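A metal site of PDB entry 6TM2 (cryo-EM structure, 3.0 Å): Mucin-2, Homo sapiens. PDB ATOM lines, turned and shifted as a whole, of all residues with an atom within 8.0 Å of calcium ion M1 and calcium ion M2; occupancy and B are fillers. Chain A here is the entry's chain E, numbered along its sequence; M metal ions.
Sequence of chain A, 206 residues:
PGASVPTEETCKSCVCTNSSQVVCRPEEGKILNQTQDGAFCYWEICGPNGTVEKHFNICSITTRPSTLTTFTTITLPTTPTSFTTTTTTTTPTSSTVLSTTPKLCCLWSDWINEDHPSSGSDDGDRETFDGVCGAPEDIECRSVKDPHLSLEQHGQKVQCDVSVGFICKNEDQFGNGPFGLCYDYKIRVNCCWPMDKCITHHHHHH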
ATOM      1  N   ILE A 112      -4.921  35.518   8.954  1.00  0.00           N
ATOM      2  CA  ILE A 112      -4.875  35.355   7.507  1.00  0.00           C
ATOM      3  C   ILE A 112      -4.223  34.018   7.213  1.00  0.00           C
ATOM      4  O   ILE A 112      -3.009  33.866   7.366  1.00  0.00           O
ATOM      5  CB  ILE A 112      -4.120  36.509   6.827  1.00  0.00           C
ATOM      6  CG1 ILE A 112      -4.817  37.840   7.110  1.00  0.00           C
ATOM      7  CG2 ILE A 112      -4.052  36.284   5.333  1.00  0.00           C
ATOM      8  CD1 ILE A 112      -3.999  39.038   6.711  1.00  0.00           C
ATOM      9  N   ASN A 113      -5.027  33.052   6.793  1.00  0.00           N
ATOM     10  CA  ASN A 113      -4.538  31.745   6.337  1.00  0.00           C
ATOM     11  C   ASN A 113      -4.944  31.630   4.876  1.00  0.00           C
ATOM     12  O   ASN A 113      -5.998  31.068   4.557  1.00  0.00           O
ATOM     13  CB  ASN A 113      -5.114  30.611   7.180  1.00  0.00           C
ATOM     14  CG  ASN A 113      -4.404  29.294   6.947  1.00  0.00           C
ATOM     15  OD1 ASN A 113      -3.397  29.225   6.231  1.00  0.00           O
ATOM     16  ND2 ASN A 113      -4.959  28.228   7.491  1.00  0.00           N
ATOM     17  N   GLU A 114      -4.115  32.153   3.986  1.00  0.00           N
ATOM     18  CA  GLU A 114      -4.425  32.201   2.564  1.00  0.00           C
ATOM     19  C   GLU A 114      -3.497  31.310   1.744  1.00  0.00           C
ATOM     20  O   GLU A 114      -3.414  31.475   0.527  1.00  0.00           O
ATOM     21  CB  GLU A 114      -4.375  33.638   2.059  1.00  0.00           C
ATOM     22  N   ASP A 115      -2.818  30.370   2.381  1.00  0.00           N
ATOM     23  CA  ASP A 115      -1.888  29.498   1.689  1.00  0.00           C
ATOM     24  C   ASP A 115      -1.769  28.215   2.509  1.00  0.00           C
ATOM     25  O   ASP A 115      -2.108  28.186   3.696  1.00  0.00           O
ATOM     26  CB  ASP A 115      -0.527  30.185   1.511  1.00  0.00           C
ATOM     27  CG  ASP A 115       0.358  29.485   0.500  1.00  0.00           C
ATOM     28  OD1 ASP A 115      -0.062  28.449  -0.067  1.00  0.00           O
ATOM     29  OD2 ASP A 115       1.481  29.984   0.250  1.00  0.00           O
ATOM     30  N   HIS A 116      -1.324  27.148   1.861  1.00  0.00           N
ATOM     31  CA  HIS A 116      -1.247  25.839   2.473  1.00  0.00           C
ATOM     32  C   HIS A 116       0.009  25.128   2.001  1.00  0.00           C
ATOM     33  O   HIS A 116       0.544  25.443   0.937  1.00  0.00           O
ATOM     34  CB  HIS A 116      -2.483  24.990   2.138  1.00  0.00           C
ATOM     35  CG  HIS A 116      -3.753  25.539   2.711  1.00  0.00           C
ATOM     36  ND1 HIS A 116      -4.082  25.403   4.036  1.00  0.00           N
ATOM     37  CD2 HIS A 116      -4.744  26.265   2.146  1.00  0.00           C
ATOM     38  CE1 HIS A 116      -5.240  25.997   4.262  1.00  0.00           C
ATOM     39  NE2 HIS A 116      -5.661  26.530   3.135  1.00  0.00           N
ATOM     40  N   PRO A 117       0.526  24.182   2.789  1.00  0.00           N
ATOM     41  CA  PRO A 117       1.664  23.382   2.303  1.00  0.00           C
ATOM     42  C   PRO A 117       1.275  22.353   1.256  1.00  0.00           C
ATOM     43  O   PRO A 117       2.037  22.105   0.319  1.00  0.00           O
ATOM     44  CB  PRO A 117       2.193  22.724   3.583  1.00  0.00           C
ATOM     45  CG  PRO A 117       1.719  23.592   4.679  1.00  0.00           C
ATOM     46  CD  PRO A 117       0.383  24.073   4.248  1.00  0.00           C
ATOM     47  N   SER A 118       0.089  21.743   1.389  1.00  0.00           N
ATOM     48  CA  SER A 118      -0.379  20.727   0.457  1.00  0.00           C
ATOM     49  C   SER A 118      -1.194  21.318  -0.695  1.00  0.00           C
ATOM     50  O   SER A 118      -2.003  20.602  -1.290  1.00  0.00           O
ATOM     51  CB  SER A 118      -1.198  19.674   1.194  1.00  0.00           C
ATOM     52  OG  SER A 118      -1.693  18.687   0.309  1.00  0.00           O
ATOM     53  N   SER A 119      -1.005  22.596  -0.995  1.00  0.00           N
ATOM     54  CA  SER A 119      -1.638  23.258  -2.134  1.00  0.00           C
ATOM     55  C   SER A 119      -0.769  24.446  -2.508  1.00  0.00           C
ATOM     56  O   SER A 119       0.260  24.715  -1.895  1.00  0.00           O
ATOM     57  CB  SER A 119      -3.076  23.687  -1.820  1.00  0.00           C
ATOM     58  OG  SER A 119      -3.905  22.562  -1.614  1.00  0.00           O
ATOM     59  N   GLY A 120      -1.198  25.173  -3.533  1.00  0.00           N
ATOM     60  CA  GLY A 120      -0.427  26.286  -4.034  1.00  0.00           C
ATOM     61  C   GLY A 120       0.703  25.841  -4.932  1.00  0.00           C
ATOM     62  O   GLY A 120       0.797  24.675  -5.342  1.00  0.00           O
ATOM     63  N   SER A 121       1.581  26.793  -5.258  1.00  0.00           N
ATOM     64  CA  SER A 121       2.726  26.492  -6.107  1.00  0.00           C
ATOM     65  C   SER A 121       3.994  27.209  -5.676  1.00  0.00           C
ATOM     66  O   SER A 121       4.967  27.224  -6.445  1.00  0.00           O
ATOM     67  CB  SER A 121       2.404  26.849  -7.565  1.00  0.00           C
ATOM     68  OG  SER A 121       1.360  26.022  -8.062  1.00  0.00           O
ATOM     69  N   ASP A 122       4.036  27.803  -4.485  1.00  0.00           N
ATOM     70  CA  ASP A 122       5.225  28.486  -4.002  1.00  0.00           C
ATOM     71  C   ASP A 122       6.163  27.597  -3.204  1.00  0.00           C
ATOM     72  O   ASP A 122       7.110  28.113  -2.595  1.00  0.00           O
ATOM     73  CB  ASP A 122       4.820  29.726  -3.177  1.00  0.00           C
ATOM     74  CG  ASP A 122       3.912  29.391  -2.006  1.00  0.00           C
ATOM     75  OD1 ASP A 122       3.499  28.218  -1.853  1.00  0.00           O
ATOM     76  OD2 ASP A 122       3.600  30.305  -1.224  1.00  0.00           O
ATOM     77  N   ASP A 123       5.904  26.279  -3.192  1.00  0.00           N
ATOM     78  CA  ASP A 123       6.763  25.244  -2.596  1.00  0.00           C
ATOM     79  C   ASP A 123       6.961  25.472  -1.103  1.00  0.00           C
ATOM     80  O   ASP A 123       8.069  25.403  -0.569  1.00  0.00           O
ATOM     81  CB  ASP A 123       8.108  25.167  -3.342  1.00  0.00           C
ATOM     82  CG  ASP A 123       8.861  23.865  -3.083  1.00  0.00           C
ATOM     83  OD1 ASP A 123       8.356  23.001  -2.354  1.00  0.00           O
ATOM     84  OD2 ASP A 123       9.990  23.721  -3.618  1.00  0.00           O
ATOM     85  N   GLY A 124       5.862  25.759  -0.398  1.00  0.00           N
ATOM     86  CA  GLY A 124       5.960  26.057   1.015  1.00  0.00           C
ATOM     87  C   GLY A 124       4.735  26.758   1.554  1.00  0.00           C
ATOM     88  O   GLY A 124       3.608  26.326   1.298  1.00  0.00           O
ATOM     89  N   ASP A 125       4.931  27.841   2.300  1.00  0.00           N
ATOM     90  CA  ASP A 125       3.805  28.570   2.888  1.00  0.00           C
ATOM     91  C   ASP A 125       4.233  30.022   3.036  1.00  0.00           C
ATOM     92  O   ASP A 125       5.214  30.308   3.730  1.00  0.00           O
ATOM     93  CB  ASP A 125       3.406  27.974   4.231  1.00  0.00           C
ATOM     94  CG  ASP A 125       2.063  28.467   4.721  1.00  0.00           C
ATOM     95  OD1 ASP A 125       1.426  29.285   4.033  1.00  0.00           O
ATOM     96  OD2 ASP A 125       1.634  28.032   5.796  1.00  0.00           O
ATOM     97  N   ARG A 126       3.503  30.925   2.389  1.00  0.00           N
ATOM     98  CA  ARG A 126       3.825  32.343   2.422  1.00  0.00           C
ATOM     99  C   ARG A 126       2.553  33.146   2.622  1.00  0.00           C
ATOM    100  O   ARG A 126       1.590  32.982   1.870  1.00  0.00           O
ATOM    101  CB  ARG A 126       4.536  32.790   1.142  1.00  0.00           C
ATOM    102  CG  ARG A 126       5.942  32.232   0.984  1.00  0.00           C
ATOM    103  CD  ARG A 126       6.613  32.669  -0.299  1.00  0.00           C
ATOM    104  NE  ARG A 126       7.947  32.086  -0.405  1.00  0.00           N
ATOM    105  CZ  ARG A 126       8.746  32.249  -1.453  1.00  0.00           C
ATOM    106  NH1 ARG A 126       8.353  32.977  -2.490  1.00  0.00           N
ATOM    107  NH2 ARG A 126       9.945  31.681  -1.471  1.00  0.00           N
ATOM    108  N   GLU A 127       2.550  34.017   3.627  1.00  0.00           N
ATOM    109  CA  GLU A 127       1.392  34.810   4.005  1.00  0.00           C
ATOM    110  C   GLU A 127       1.784  36.279   4.001  1.00  0.00           C
ATOM    111  O   GLU A 127       2.646  36.690   4.776  1.00  0.00           O
ATOM    112  CB  GLU A 127       0.869  34.392   5.392  1.00  0.00           C
ATOM    113  CG  GLU A 127       0.298  32.993   5.438  1.00  0.00           C
ATOM    114  CD  GLU A 127      -0.989  32.876   4.660  1.00  0.00           C
ATOM    115  OE1 GLU A 127      -1.755  33.855   4.604  1.00  0.00           O
ATOM    116  OE2 GLU A 127      -1.234  31.796   4.094  1.00  0.00           O
ATOM    117  N   ARG A 142       1.996  32.534  14.010  1.00  0.00           N
ATOM    118  CA  ARG A 142       1.529  31.343  14.734  1.00  0.00           C
ATOM    119  C   ARG A 142       1.113  30.258  13.758  1.00  0.00           C
ATOM    120  O   ARG A 142       1.114  30.441  12.542  1.00  0.00           O
ATOM    121  CB  ARG A 142       0.376  31.671  15.682  1.00  0.00           C
ATOM    122  CG  ARG A 142       0.774  32.595  16.802  1.00  0.00           C
ATOM    123  CD  ARG A 142       1.744  31.872  17.713  1.00  0.00           C
ATOM    124  NE  ARG A 142       2.240  32.709  18.800  1.00  0.00           N
ATOM    125  CZ  ARG A 142       1.649  32.811  19.979  1.00  0.00           C
ATOM    126  NH1 ARG A 142       0.525  32.145  20.225  1.00  0.00           N
ATOM    127  NH2 ARG A 142       2.169  33.588  20.913  1.00  0.00           N
ATOM    128  N   SER A 143       0.756  29.108  14.319  1.00  0.00           N
ATOM    129  CA  SER A 143       0.351  27.937  13.544  1.00  0.00           C
ATOM    130  C   SER A 143      -1.147  27.715  13.667  1.00  0.00           C
ATOM    131  O   SER A 143      -1.799  28.179  14.594  1.00  0.00           O
ATOM    132  CB  SER A 143       1.081  26.680  14.013  1.00  0.00           C
ATOM    133  OG  SER A 143       0.654  25.546  13.271  1.00  0.00           O
ATOM    134  N   VAL A 144      -1.689  26.978  12.703  1.00  0.00           N
ATOM    135  CA  VAL A 144      -3.121  26.791  12.625  1.00  0.00           C
ATOM    136  C   VAL A 144      -3.592  25.762  13.643  1.00  0.00           C
ATOM    137  O   VAL A 144      -4.469  26.041  14.478  1.00  0.00           O
ATOM    138  CB  VAL A 144      -3.528  26.387  11.203  1.00  0.00           C
ATOM    139  CG1 VAL A 144      -4.997  26.080  11.146  1.00  0.00           C
ATOM    140  CG2 VAL A 144      -3.198  27.495  10.258  1.00  0.00           C
ATOM    141  N   PHE A 166       5.601  36.499   5.681  1.00  0.00           N
ATOM    142  CA  PHE A 166       6.001  35.184   6.169  1.00  0.00           C
ATOM    143  C   PHE A 166       6.507  34.357   5.003  1.00  0.00           C
ATOM    144  O   PHE A 166       5.924  34.371   3.915  1.00  0.00           O
ATOM    145  CB  PHE A 166       4.839  34.481   6.858  1.00  0.00           C
ATOM    146  CG  PHE A 166       5.178  33.132   7.399  1.00  0.00           C
ATOM    147  CD1 PHE A 166       5.934  33.001   8.545  1.00  0.00           C
ATOM    148  CD2 PHE A 166       4.750  31.984   6.756  1.00  0.00           C
ATOM    149  CE1 PHE A 166       6.267  31.766   9.040  1.00  0.00           C
ATOM    150  CE2 PHE A 166       5.072  30.745   7.244  1.00  0.00           C
ATOM    151  CZ  PHE A 166       5.834  30.634   8.383  1.00  0.00           C
ATOM    152  N   CYS A 168       8.037  30.348   4.301  1.00  0.00           N
ATOM    153  CA  CYS A 168       8.503  29.006   4.610  1.00  0.00           C
ATOM    154  C   CYS A 168       8.775  28.304   3.290  1.00  0.00           C
ATOM    155  O   CYS A 168       7.945  28.369   2.373  1.00  0.00           O
ATOM    156  CB  CYS A 168       7.478  28.208   5.447  1.00  0.00           C
ATOM    157  SG  CYS A 168       8.006  26.576   6.043  1.00  0.00           S
ATOM    158  N   ASN A 170       9.915  24.601   1.510  1.00  0.00           N
ATOM    159  CA  ASN A 170      10.000  23.155   1.770  1.00  0.00           C
ATOM    160  C   ASN A 170      11.412  22.618   1.605  1.00  0.00           C
ATOM    161  O   ASN A 170      11.744  21.585   2.203  1.00  0.00           O
ATOM    162  CB  ASN A 170       9.067  22.363   0.855  1.00  0.00           C
ATOM    163  CG  ASN A 170       7.621  22.483   1.245  1.00  0.00           C
ATOM    164  OD1 ASN A 170       7.288  22.486   2.418  1.00  0.00           O
ATOM    165  ND2 ASN A 170       6.751  22.541   0.248  1.00  0.00           N
ATOM    166  N   TYR A 183       4.678  23.436   8.094  1.00  0.00           N
ATOM    167  CA  TYR A 183       3.441  23.357   8.845  1.00  0.00           C
ATOM    168  C   TYR A 183       2.497  24.423   8.298  1.00  0.00           C
ATOM    169  O   TYR A 183       2.859  25.219   7.425  1.00  0.00           O
ATOM    170  CB  TYR A 183       3.705  23.517  10.337  1.00  0.00           C
ATOM    171  CG  TYR A 183       4.531  22.396  10.940  1.00  0.00           C
ATOM    172  CD1 TYR A 183       4.589  21.140  10.350  1.00  0.00           C
ATOM    173  CD2 TYR A 183       5.332  22.620  12.047  1.00  0.00           C
ATOM    174  CE1 TYR A 183       5.359  20.142  10.882  1.00  0.00           C
ATOM    175  CE2 TYR A 183       6.120  21.635  12.573  1.00  0.00           C
ATOM    176  CZ  TYR A 183       6.125  20.390  11.986  1.00  0.00           C
ATOM    177  OH  TYR A 183       6.913  19.393  12.505  1.00  0.00           O
ATOM    178  N   ASP A 184       1.276  24.461   8.793  1.00  0.00           N
ATOM    179  CA  ASP A 184       0.279  25.392   8.308  1.00  0.00           C
ATOM    180  C   ASP A 184       0.260  26.600   9.242  1.00  0.00           C
ATOM    181  O   ASP A 184      -0.041  26.449  10.435  1.00  0.00           O
ATOM    182  CB  ASP A 184      -1.086  24.717   8.230  1.00  0.00           C
ATOM    183  CG  ASP A 184      -2.097  25.510   7.436  1.00  0.00           C
ATOM    184  OD1 ASP A 184      -1.772  26.608   6.937  1.00  0.00           O
ATOM    185  OD2 ASP A 184      -3.237  25.023   7.307  1.00  0.00           O
ATOM    186  N   TYR A 185       0.585  27.770   8.713  1.00  0.00           N
ATOM    187  CA  TYR A 185       0.774  28.976   9.500  1.00  0.00           C
ATOM    188  C   TYR A 185      -0.308  30.006   9.178  1.00  0.00           C
ATOM    189  O   TYR A 185      -1.029  29.893   8.188  1.00  0.00           O
ATOM    190  CB  TYR A 185       2.163  29.564   9.227  1.00  0.00           C
ATOM    191  CG  TYR A 185       3.321  28.752   9.764  1.00  0.00           C
ATOM    192  CD1 TYR A 185       3.755  28.914  11.071  1.00  0.00           C
ATOM    193  CD2 TYR A 185       3.953  27.805   8.979  1.00  0.00           C
ATOM    194  CE1 TYR A 185       4.816  28.193  11.563  1.00  0.00           C
ATOM    195  CE2 TYR A 185       5.008  27.064   9.464  1.00  0.00           C
ATOM    196  CZ  TYR A 185       5.437  27.265  10.755  1.00  0.00           C
ATOM    197  OH  TYR A 185       6.487  26.540  11.240  1.00  0.00           O
ATOM    198  N   LYS A 186      -0.391  31.018  10.032  1.00  0.00           N
ATOM    199  CA  LYS A 186      -1.338  32.109   9.896  1.00  0.00           C
ATOM    200  C   LYS A 186      -0.774  33.320  10.619  1.00  0.00           C
ATOM    201  O   LYS A 186       0.036  33.185  11.528  1.00  0.00           O
ATOM    202  CB  LYS A 186      -2.713  31.720  10.443  1.00  0.00           C
ATOM    203  CG  LYS A 186      -2.721  31.448  11.937  1.00  0.00           C
ATOM    204  CD  LYS A 186      -4.083  31.017  12.415  1.00  0.00           C
ATOM    205  CE  LYS A 186      -4.068  30.791  13.903  1.00  0.00           C
ATOM    206  NZ  LYS A 186      -5.403  30.377  14.397  1.00  0.00           N
ATOM    207  N   ILE A 187      -1.181  34.530  10.190  1.00  0.00           N
ATOM    208  CA  ILE A 187      -0.595  35.769  10.701  1.00  0.00           C
ATOM    209  C   ILE A 187      -1.656  36.825  10.997  1.00  0.00           C
ATOM    210  O   ILE A 187      -2.754  36.829  10.437  1.00  0.00           O
ATOM    211  CB  ILE A 187       0.452  36.390   9.734  1.00  0.00           C
ATOM    212  CG1 ILE A 187      -0.179  36.721   8.389  1.00  0.00           C
ATOM    213  CG2 ILE A 187       1.692  35.510   9.598  1.00  0.00           C
ATOM    214  CD1 ILE A 187       0.710  37.564   7.498  1.00  0.00           C
HETATM  215 CA    CA M   1      -0.902  28.949   5.818  1.00  0.00          CA
HETATM  216 CA    CA M   2       1.578  26.756  -1.101  1.00  0.00          CA
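The side-chain amide oxygen (OD1) of Asn 113 binds calcium ion M1 (2.5 Å).
The backbone carbonyl oxygen (O) of Tyr 185 binds calcium ion M1 (2.6 Å).
The backbone carbonyl oxygen (O) of Asp 115 is bound to calcium ion M1 (2.6 Å).
The side-chain carboxylate (OD2) of Asp 125 binds calcium ion M1 (2.7 Å).
OD1 of Asp 184 binds calcium ion M1 (2.7 Å).
Slightly farther from calcium ion M1 lies OD1 of Asp 125 (3.0 Å).
Gly 120 touches calcium ion M2 (CA to CA, 3.6 Å).
O of Gly 124 touches calcium ion M2, at 3.2 Å.
Within 4 Å of calcium ion M2: Asp 115, His 116, Ser 119, Gly 120, Asp 122 and Gly 124.
Along chain A the residues within 4 Å of calcium ion M2 span positions 115 to 124.
The side-chain carboxylate of Glu 127 sits at hydrogen-bond distance from the backbone NH of Asp 115, at 2.7 Å.
N of Arg 126 sits at hydrogen-bond distance from OD2 of Asp 115, at 3.1 Å.
OD2 of Asp 184 lies within hydrogen-bond range of ND1 of His 116, 3.4 Å away.
O of Asp 125 lies within hydrogen-bond range of N of Cys 168, 2.9 Å away.
The backbone carbonyl oxygen (O) of Asp 184 is in hydrogen-bond range of the backbone NH (N) of Val 144, at 2.9 Å.
The side-chain hydroxyl of Ser 143 is in hydrogen-bond range of the backbone carbonyl oxygen of Asp 184, at 3.1 Å.
The backbone NH (N) of Gly 124 lies close to the side-chain amide nitrogen (ND2) of Asn 170 (3.4 Å).
The side-chain carboxylate (OE2) of Glu 127 is in hydrogen-bond range of the backbone NH (N) of Glu 114 (2.9 Å).
Calcium ion M2 is bound by OD1 of Asp 122 (2.5 Å).
Calcium ion M2 is bound by the backbone carbonyl oxygen (O) of Ser 119, 2.6 Å away.
OD1 of Asp 115 binds calcium ion M2, at 2.6 Å.
Calcium ion M2 is bound by O of His 116, at 2.6 Å.
Calcium ion M2 has four donor atoms within binding distance.
Residues that only touch calcium ion M1: Glu 127 (3.3 Å).
Within 4 Å of calcium ion M1: Asn 113, Asp 115, Asp 125, Glu 127, Asp 184 and Tyr 185.
Along chain A the residues within 4 Å of calcium ion M1 span positions 113 to 185.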
